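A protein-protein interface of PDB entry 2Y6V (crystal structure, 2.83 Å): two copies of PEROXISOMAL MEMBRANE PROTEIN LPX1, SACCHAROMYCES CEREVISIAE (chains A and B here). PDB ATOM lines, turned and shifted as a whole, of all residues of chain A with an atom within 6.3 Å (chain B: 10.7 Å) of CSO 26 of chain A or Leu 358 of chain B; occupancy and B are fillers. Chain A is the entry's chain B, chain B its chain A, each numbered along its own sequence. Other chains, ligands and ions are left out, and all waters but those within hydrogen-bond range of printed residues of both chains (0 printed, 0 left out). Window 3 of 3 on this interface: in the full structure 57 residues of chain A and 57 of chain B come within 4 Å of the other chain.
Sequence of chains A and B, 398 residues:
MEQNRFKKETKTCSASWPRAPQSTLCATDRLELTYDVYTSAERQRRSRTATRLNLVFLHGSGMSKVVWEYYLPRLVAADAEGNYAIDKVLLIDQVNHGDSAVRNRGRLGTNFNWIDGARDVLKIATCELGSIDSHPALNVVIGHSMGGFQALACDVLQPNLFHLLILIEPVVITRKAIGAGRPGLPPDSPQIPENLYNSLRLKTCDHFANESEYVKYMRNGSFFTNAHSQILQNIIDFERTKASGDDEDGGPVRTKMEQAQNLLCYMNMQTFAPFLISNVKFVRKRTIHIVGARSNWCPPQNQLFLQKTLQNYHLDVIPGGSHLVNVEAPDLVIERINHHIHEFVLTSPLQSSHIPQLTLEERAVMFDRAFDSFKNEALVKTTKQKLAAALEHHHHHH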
ATOM      1  N   THR A  24      -8.961   8.214  19.277  1.00  0.00           N
ATOM      2  CA  THR A  24      -8.955   8.375  20.730  1.00  0.00           C
ATOM      3  C   THR A  24      -7.552   8.266  21.231  1.00  0.00           C
ATOM      4  O   THR A  24      -6.697   7.730  20.557  1.00  0.00           O
ATOM      5  CB  THR A  24      -9.785   7.296  21.448  1.00  0.00           C
ATOM      6  OG1 THR A  24      -9.236   6.003  21.171  1.00  0.00           O
ATOM      7  CG2 THR A  24     -11.219   7.335  20.987  1.00  0.00           C
ATOM      8  N   LEU A  25      -7.335   8.778  22.437  1.00  0.00           N
ATOM      9  CA  LEU A  25      -6.019   8.776  23.082  1.00  0.00           C
ATOM     10  C   LEU A  25      -5.593   7.351  23.440  1.00  0.00           C
ATOM     11  O   LEU A  25      -4.428   6.985  23.249  1.00  0.00           O
ATOM     12  CB  LEU A  25      -6.059   9.653  24.336  1.00  0.00           C
ATOM     13  CG  LEU A  25      -4.735  10.166  24.876  1.00  0.00           C
ATOM     14  CD1 LEU A  25      -3.996  10.960  23.776  1.00  0.00           C
ATOM     15  CD2 LEU A  25      -4.983  11.030  26.110  1.00  0.00           C
ATOM     16  N   CSO A  26      -6.535   6.565  23.964  1.00  0.00           N
ATOM     17  CA  CSO A  26      -6.356   5.111  24.128  1.00  0.00           C
ATOM     18  CB  CSO A  26      -6.378   4.690  25.601  1.00  0.00           C
ATOM     19  SG  CSO A  26      -5.200   5.582  26.626  1.00  0.00           S
ATOM     20  C   CSO A  26      -7.358   4.235  23.337  1.00  0.00           C
ATOM     21  O   CSO A  26      -8.502   4.595  23.133  1.00  0.00           O
ATOM     22  OD  CSO A  26      -3.685   4.625  26.895  1.00  0.00           O
ATOM     23  N   ALA A  27      -6.910   3.059  22.913  1.00  0.00           N
ATOM     24  CA  ALA A  27      -7.745   2.157  22.112  1.00  0.00           C
ATOM     25  C   ALA A  27      -9.004   1.683  22.878  1.00  0.00           C
ATOM     26  O   ALA A  27     -10.061   1.565  22.304  1.00  0.00           O
ATOM     27  CB  ALA A  27      -6.920   0.984  21.629  1.00  0.00           C
ATOM     28  N   THR A  28      -8.914   1.456  24.186  1.00  0.00           N
ATOM     29  CA  THR A  28     -10.116   1.137  24.991  1.00  0.00           C
ATOM     30  C   THR A  28     -11.105   2.305  25.289  1.00  0.00           C
ATOM     31  O   THR A  28     -12.184   2.076  25.834  1.00  0.00           O
ATOM     32  CB  THR A  28      -9.726   0.508  26.322  1.00  0.00           C
ATOM     33  OG1 THR A  28      -8.682   1.287  26.923  1.00  0.00           O
ATOM     34  CG2 THR A  28      -9.280  -0.910  26.080  1.00  0.00           C
ATOM     35  N   ASP A  29     -10.734   3.540  24.948  1.00  0.00           N
ATOM     36  CA  ASP A  29     -11.652   4.681  25.087  1.00  0.00           C
ATOM     37  C   ASP A  29     -12.800   4.602  24.108  1.00  0.00           C
ATOM     38  O   ASP A  29     -12.674   3.998  23.035  1.00  0.00           O
ATOM     39  CB  ASP A  29     -10.931   5.994  24.844  1.00  0.00           C
ATOM     40  CG  ASP A  29      -9.908   6.304  25.891  1.00  0.00           C
ATOM     41  OD1 ASP A  29      -9.978   5.736  26.966  1.00  0.00           O
ATOM     42  OD2 ASP A  29      -9.044   7.137  25.625  1.00  0.00           O
ATOM     43  N   ARG A  30     -13.917   5.215  24.483  1.00  0.00           N
ATOM     44  CA  ARG A  30     -15.107   5.256  23.624  1.00  0.00           C
ATOM     45  C   ARG A  30     -15.691   6.655  23.566  1.00  0.00           C
ATOM     46  O   ARG A  30     -15.893   7.296  24.603  1.00  0.00           O
ATOM     47  CB  ARG A  30     -16.138   4.275  24.124  1.00  0.00           C
ATOM     48  CG  ARG A  30     -15.715   2.824  23.909  1.00  0.00           C
ATOM     49  CD  ARG A  30     -15.537   2.512  22.459  1.00  0.00           C
ATOM     50  NE  ARG A  30     -15.340   1.108  22.185  1.00  0.00           N
ATOM     51  CZ  ARG A  30     -14.174   0.484  22.275  1.00  0.00           C
ATOM     52  NH1 ARG A  30     -13.090   1.149  22.672  1.00  0.00           N
ATOM     53  NH2 ARG A  30     -14.087  -0.809  21.974  1.00  0.00           N
ATOM     54  N   GLY A 106     -10.433  14.490  27.503  1.00  0.00           N
ATOM     55  CA  GLY A 106      -9.506  13.464  27.908  1.00  0.00           C
ATOM     56  C   GLY A 106      -9.446  12.261  27.000  1.00  0.00           C
ATOM     57  O   GLY A 106      -8.509  11.495  27.084  1.00  0.00           O
ATOM     58  N   ARG A 107     -10.409  12.092  26.103  1.00  0.00           N
ATOM     59  CA  ARG A 107     -10.424  10.911  25.244  1.00  0.00           C
ATOM     60  C   ARG A 107     -10.027  11.105  23.795  1.00  0.00           C
ATOM     61  O   ARG A 107      -9.703  10.121  23.141  1.00  0.00           O
ATOM     62  CB  ARG A 107     -11.796  10.275  25.235  1.00  0.00           C
ATOM     63  CG  ARG A 107     -12.422   9.977  26.568  1.00  0.00           C
ATOM     64  CD  ARG A 107     -13.912   9.844  26.319  1.00  0.00           C
ATOM     65  NE  ARG A 107     -14.739   9.630  27.503  1.00  0.00           N
ATOM     66  CZ  ARG A 107     -16.071   9.735  27.507  1.00  0.00           C
ATOM     67  NH1 ARG A 107     -16.739  10.051  26.404  1.00  0.00           N
ATOM     68  NH2 ARG A 107     -16.744   9.515  28.624  1.00  0.00           N
ATOM     69  N   ILE B 132     -15.121  -3.538  25.102  1.00  0.00           N
ATOM     70  CA  ILE B 132     -13.763  -3.326  25.645  1.00  0.00           C
ATOM     71  C   ILE B 132     -13.124  -4.675  26.021  1.00  0.00           C
ATOM     72  O   ILE B 132     -11.895  -4.865  25.940  1.00  0.00           O
ATOM     73  CB  ILE B 132     -13.828  -2.432  26.889  1.00  0.00           C
ATOM     74  CG1 ILE B 132     -14.334  -1.026  26.511  1.00  0.00           C
ATOM     75  CG2 ILE B 132     -12.472  -2.317  27.558  1.00  0.00           C
ATOM     76  CD1 ILE B 132     -14.654  -0.101  27.765  1.00  0.00           C
ATOM     77  N   HIS B 135     -10.818  -6.535  23.368  1.00  0.00           N
ATOM     78  CA  HIS B 135      -9.468  -5.995  23.076  1.00  0.00           C
ATOM     79  C   HIS B 135      -8.373  -6.772  23.820  1.00  0.00           C
ATOM     80  O   HIS B 135      -8.535  -7.089  25.012  1.00  0.00           O
ATOM     81  CB  HIS B 135      -9.402  -4.498  23.437  1.00  0.00           C
ATOM     82  CG  HIS B 135      -8.057  -3.882  23.220  1.00  0.00           C
ATOM     83  ND1 HIS B 135      -7.654  -3.368  22.000  1.00  0.00           N
ATOM     84  CD2 HIS B 135      -7.010  -3.707  24.072  1.00  0.00           C
ATOM     85  CE1 HIS B 135      -6.413  -2.910  22.108  1.00  0.00           C
ATOM     86  NE2 HIS B 135      -6.000  -3.097  23.360  1.00  0.00           N
ATOM     87  N   SER B 352      -1.506  -4.111  22.696  1.00  0.00           N
ATOM     88  CA  SER B 352      -1.264  -3.447  23.993  1.00  0.00           C
ATOM     89  C   SER B 352      -1.776  -4.232  25.212  1.00  0.00           C
ATOM     90  O   SER B 352      -1.082  -4.313  26.221  1.00  0.00           O
ATOM     91  CB  SER B 352      -1.824  -1.998  23.993  1.00  0.00           C
ATOM     92  OG  SER B 352      -3.193  -1.958  24.404  1.00  0.00           O
ATOM     93  N   SER B 353      -2.978  -4.792  25.111  1.00  0.00           N
ATOM     94  CA  SER B 353      -3.561  -5.708  26.135  1.00  0.00           C
ATOM     95  C   SER B 353      -3.943  -5.059  27.477  1.00  0.00           C
ATOM     96  O   SER B 353      -4.844  -5.549  28.169  1.00  0.00           O
ATOM     97  CB  SER B 353      -2.697  -6.985  26.355  1.00  0.00           C
ATOM     98  OG  SER B 353      -1.298  -6.768  26.197  1.00  0.00           O
ATOM     99  N   PRO B 356      -5.944   1.085  31.011  1.00  0.00           N
ATOM    100  CA  PRO B 356      -4.871   1.895  31.615  1.00  0.00           C
ATOM    101  C   PRO B 356      -5.442   3.014  32.476  1.00  0.00           C
ATOM    102  O   PRO B 356      -5.741   4.082  31.923  1.00  0.00           O
ATOM    103  CB  PRO B 356      -4.174   2.526  30.371  1.00  0.00           C
ATOM    104  CG  PRO B 356      -5.315   2.618  29.274  1.00  0.00           C
ATOM    105  CD  PRO B 356      -6.509   1.773  29.825  1.00  0.00           C
ATOM    106  N   GLN B 357      -5.628   2.795  33.776  1.00  0.00           N
ATOM    107  CA  GLN B 357      -6.240   3.825  34.616  1.00  0.00           C
ATOM    108  C   GLN B 357      -5.458   5.136  34.436  1.00  0.00           C
ATOM    109  O   GLN B 357      -4.370   5.307  35.008  1.00  0.00           O
ATOM    110  CB  GLN B 357      -6.259   3.418  36.106  1.00  0.00           C
ATOM    111  CG  GLN B 357      -7.086   2.139  36.476  1.00  0.00           C
ATOM    112  CD  GLN B 357      -6.221   0.907  36.882  1.00  0.00           C
ATOM    113  OE1 GLN B 357      -5.066   0.762  36.462  1.00  0.00           O
ATOM    114  NE2 GLN B 357      -6.801   0.018  37.694  1.00  0.00           N
ATOM    115  N   LEU B 358      -5.976   6.041  33.603  1.00  0.00           N
ATOM    116  CA  LEU B 358      -5.293   7.314  33.363  1.00  0.00           C
ATOM    117  C   LEU B 358      -6.180   8.486  33.795  1.00  0.00           C
ATOM    118  O   LEU B 358      -7.379   8.519  33.486  1.00  0.00           O
ATOM    119  CB  LEU B 358      -4.902   7.484  31.903  1.00  0.00           C
ATOM    120  CG  LEU B 358      -3.684   6.740  31.377  1.00  0.00           C
ATOM    121  CD1 LEU B 358      -3.743   6.606  29.841  1.00  0.00           C
ATOM    122  CD2 LEU B 358      -2.410   7.432  31.773  1.00  0.00           C
ATOM    123  N   THR B 359      -5.589   9.431  34.520  1.00  0.00           N
ATOM    124  CA  THR B 359      -6.306  10.592  35.025  1.00  0.00           C
ATOM    125  C   THR B 359      -6.417  11.601  33.909  1.00  0.00           C
ATOM    126  O   THR B 359      -5.682  11.505  32.942  1.00  0.00           O
ATOM    127  CB  THR B 359      -5.607  11.237  36.256  1.00  0.00           C
ATOM    128  OG1 THR B 359      -4.380  11.888  35.871  1.00  0.00           O
ATOM    129  CG2 THR B 359      -5.319  10.187  37.305  1.00  0.00           C
ATOM    130  N   LEU B 360      -7.345  12.546  34.045  1.00  0.00           N
ATOM    131  CA  LEU B 360      -7.497  13.660  33.106  1.00  0.00           C
ATOM    132  C   LEU B 360      -6.205  14.426  32.910  1.00  0.00           C
ATOM    133  O   LEU B 360      -5.914  14.894  31.818  1.00  0.00           O
ATOM    134  CB  LEU B 360      -8.565  14.655  33.579  1.00  0.00           C
ATOM    135  CG  LEU B 360      -9.978  14.543  33.003  1.00  0.00           C
ATOM    136  CD1 LEU B 360     -10.449  13.064  32.818  1.00  0.00           C
ATOM    137  CD2 LEU B 360     -10.953  15.340  33.869  1.00  0.00           C
ATOM    138  N   GLU B 361      -5.433  14.558  33.981  1.00  0.00           N
ATOM    139  CA  GLU B 361      -4.174  15.303  33.961  1.00  0.00           C
ATOM    140  C   GLU B 361      -3.085  14.515  33.223  1.00  0.00           C
ATOM    141  O   GLU B 361      -2.364  15.067  32.395  1.00  0.00           O
ATOM    142  CB  GLU B 361      -3.728  15.614  35.385  1.00  0.00           C
ATOM    143  CG  GLU B 361      -4.634  16.588  36.171  1.00  0.00           C
ATOM    144  CD  GLU B 361      -5.977  15.998  36.624  1.00  0.00           C
ATOM    145  OE1 GLU B 361      -6.027  14.876  37.167  1.00  0.00           O
ATOM    146  OE2 GLU B 361      -7.001  16.686  36.430  1.00  0.00           O
ATOM    147  N   GLU B 362      -2.994  13.221  33.508  1.00  0.00           N
ATOM    148  CA  GLU B 362      -2.133  12.326  32.748  1.00  0.00           C
ATOM    149  C   GLU B 362      -2.477  12.349  31.239  1.00  0.00           C
ATOM    150  O   GLU B 362      -1.589  12.400  30.389  1.00  0.00           O
ATOM    151  CB  GLU B 362      -2.204  10.908  33.351  1.00  0.00           C
ATOM    152  CG  GLU B 362      -1.523  10.823  34.722  1.00  0.00           C
ATOM    153  CD  GLU B 362      -1.573   9.465  35.375  1.00  0.00           C
ATOM    154  OE1 GLU B 362      -2.666   8.895  35.449  1.00  0.00           O
ATOM    155  OE2 GLU B 362      -0.528   8.972  35.848  1.00  0.00           O
ATOM    156  N   ARG B 363      -3.768  12.358  30.922  1.00  0.00           N
ATOM    157  CA  ARG B 363      -4.233  12.317  29.535  1.00  0.00           C
ATOM    158  C   ARG B 363      -3.888  13.593  28.801  1.00  0.00           C
ATOM    159  O   ARG B 363      -3.556  13.548  27.635  1.00  0.00           O
ATOM    160  CB  ARG B 363      -5.744  12.040  29.463  1.00  0.00           C
ATOM    161  CG  ARG B 363      -6.118  10.591  29.697  1.00  0.00           C
ATOM    162  CD  ARG B 363      -7.576  10.413  30.011  1.00  0.00           C
ATOM    163  NE  ARG B 363      -7.902   9.000  30.148  1.00  0.00           N
ATOM    164  CZ  ARG B 363      -8.136   8.169  29.137  1.00  0.00           C
ATOM    165  NH1 ARG B 363      -8.112   8.603  27.880  1.00  0.00           N
ATOM    166  NH2 ARG B 363      -8.394   6.892  29.383  1.00  0.00           N
ATOM    167  N   ALA B 364      -3.957  14.731  29.478  1.00  0.00           N
ATOM    168  CA  ALA B 364      -3.676  16.028  28.836  1.00  0.00           C
ATOM    169  C   ALA B 364      -2.196  16.168  28.490  1.00  0.00           C
ATOM    170  O   ALA B 364      -1.834  16.834  27.524  1.00  0.00           O
ATOM    171  CB  ALA B 364      -4.124  17.167  29.712  1.00  0.00           C
ATOM    172  N   VAL B 365      -1.351  15.527  29.301  1.00  0.00           N
ATOM    173  CA  VAL B 365       0.073  15.505  29.100  1.00  0.00           C
ATOM    174  C   VAL B 365       0.374  14.611  27.917  1.00  0.00           C
ATOM    175  O   VAL B 365       1.181  14.983  27.072  1.00  0.00           O
ATOM    176  CB  VAL B 365       0.822  15.014  30.398  1.00  0.00           C
ATOM    177  CG1 VAL B 365       2.316  14.648  30.145  1.00  0.00           C
ATOM    178  CG2 VAL B 365       0.732  16.067  31.501  1.00  0.00           C
ATOM    179  N   MET B 366      -0.268  13.438  27.858  1.00  0.00           N
ATOM    180  CA  MET B 366      -0.046  12.473  26.754  1.00  0.00           C
ATOM    181  C   MET B 366      -0.458  13.080  25.420  1.00  0.00           C
ATOM    182  O   MET B 366       0.236  12.936  24.420  1.00  0.00           O
ATOM    183  CB  MET B 366      -0.810  11.150  26.984  1.00  0.00           C
ATOM    184  CG  MET B 366      -0.172  10.259  28.048  1.00  0.00           C
ATOM    185  SD  MET B 366      -1.041   8.671  28.375  1.00  0.00           S
ATOM    186  CE  MET B 366      -0.859   7.931  26.713  1.00  0.00           C
ATOM    187  N   PHE B 367      -1.601  13.759  25.435  1.00  0.00           N
ATOM    188  CA  PHE B 367      -2.157  14.365  24.249  1.00  0.00           C
ATOM    189  C   PHE B 367      -1.278  15.429  23.658  1.00  0.00           C
ATOM    190  O   PHE B 367      -1.065  15.415  22.441  1.00  0.00           O
ATOM    191  CB  PHE B 367      -3.515  14.984  24.512  1.00  0.00           C
ATOM    192  CG  PHE B 367      -4.073  15.633  23.321  1.00  0.00           C
ATOM    193  CD1 PHE B 367      -4.805  14.901  22.392  1.00  0.00           C
ATOM    194  CD2 PHE B 367      -3.799  16.961  23.065  1.00  0.00           C
ATOM    195  CE1 PHE B 367      -5.298  15.511  21.236  1.00  0.00           C
ATOM    196  CE2 PHE B 367      -4.289  17.587  21.920  1.00  0.00           C
ATOM    197  CZ  PHE B 367      -5.035  16.855  21.002  1.00  0.00           C
ATOM    198  N   ARG B 369       1.774  15.916  23.916  1.00  0.00           N
ATOM    199  CA  ARG B 369       2.906  15.250  23.357  1.00  0.00           C
ATOM    200  C   ARG B 369       2.538  14.568  22.032  1.00  0.00           C
ATOM    201  O   ARG B 369       3.300  14.637  21.084  1.00  0.00           O
ATOM    202  CB  ARG B 369       3.425  14.265  24.404  1.00  0.00           C
ATOM    203  CG  ARG B 369       4.766  13.679  24.108  1.00  0.00           C
ATOM    204  CD  ARG B 369       4.989  12.469  24.984  1.00  0.00           C
ATOM    205  NE  ARG B 369       5.135  12.876  26.371  1.00  0.00           N
ATOM    206  CZ  ARG B 369       4.703  12.196  27.429  1.00  0.00           C
ATOM    207  NH1 ARG B 369       4.037  11.042  27.301  1.00  0.00           N
ATOM    208  NH2 ARG B 369       4.925  12.705  28.635  1.00  0.00           N
ATOM    209  N   ALA B 370       1.376  13.921  21.968  1.00  0.00           N
ATOM    210  CA  ALA B 370       0.883  13.317  20.727  1.00  0.00           C
ATOM    211  C   ALA B 370       0.677  14.372  19.648  1.00  0.00           C
ATOM    212  O   ALA B 370       1.078  14.173  18.508  1.00  0.00           O
ATOM    213  CB  ALA B 370      -0.403  12.581  20.982  1.00  0.00           C
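Of chain B, only Pro 356 and Leu 358 come within 4 Å of CSO 26 of chain A. Leu 358 of chain B touches just one residue of chain A: CSO 26. No residue of chain B comes within 4 Å of Thr 24 of chain A. Leu 25 of chain A touches just these residues of chain B: Arg 363 and Phe 367. Printed residues of chain A within 4 Å of His 135 of chain B: Ala 27 (3.96 Å). Of the printed residues of chain A, Phe 367 of chain B touches Leu 25 (3.9 Å). Of the printed residues of chain A, Arg 363 of chain B touches Leu 25 (3.3 Å), Asp 29 (2.8 Å) and Gly 106 (3.0 Å). Of the printed residues of chain B, Gly 106 of chain A touches Arg 363 (3.0 Å). Of the printed residues of chain A, Ile 132 of chain B touches Thr 28 (3.8 Å). Ala 370 of chain B touches none of the printed residues of chain A. Ala 364 of chain B touches none of the printed residues of chain A. The nearest printed residue of chain A that does not touch Pro 356 of chain B is Asp 29 of chain A (6.0 Å).
Hydrophobic or aromatic side chains of chain A that line the printed part of chain B: Leu 25 and Ala 27. Of the 18 printed residues of chain B, 6 touch a printed residue of chain A. Hydrophobic or aromatic side chains of chain B within 4 Å of the printed part of chain A: Ile 132, His 135, Pro 356 and Leu 358. Among the printed residues, 9 pairs touch across the chains. Among the printed residues, Asp or Glu carboxylates within 4 Å of a Lys or Arg side-chain nitrogen of the other chain: Asp 29 of chain A with Arg 363 of chain B.
Leu 25 of chain A touches Arg 363 of chain B. CA of Phe 367 of chain B touches CD1 of Leu 25 of chain A, at 3.9 Å. CG of Pro 356 of chain B touches OD of CSO 26 of chain A, at 3.5 Å. CSO 26 of chain A touches Leu 358 of chain B (OD to CD1, 3.6 Å). His 135 of chain B touches Ala 27 of chain A (CE1 to CB, 3.96 Å). Thr 28 of chain A touches Ile 132 of chain B (CG2 to CG2, 3.8 Å). CD of Pro 356 of chain B touches OG1 of Thr 28 of chain A, at 3.7 Å.
No position is printed for both chains.
O of Gly 106 of chain A is in hydrogen-bond range of NH1 of Arg 363 of chain B, 3.0 Å away. The side-chain carboxylate of Asp 29 of chain A lies within salt-bridge range of the guanidinium group of Arg 363 of chain B (2.8 Å).
The backbone carbonyl oxygen of Leu 358 of chain B sits at hydrogen-bond distance from the guanidinium group of Arg 363 of chain B (3.4 Å). O of Thr 28 of chain A is in hydrogen-bond range of NH1 of Arg 30 of chain A (3.4 Å). The backbone carbonyl oxygen of Ala 27 of chain A sits at hydrogen-bond distance from the guanidinium group of Arg 30 of chain A (3.1 Å). The side-chain hydroxyl (OG1) of Thr 24 of chain A lies within hydrogen-bond range of O of CSO 26 of chain A (2.5 Å). NE2 of His 135 of chain B lies within hydrogen-bond range of OG of Ser 352 of chain B (3.2 Å). N of CSO 26 of chain A lies within hydrogen-bond range of the side-chain carboxylate of Asp 29 of chain A (3.1 Å).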
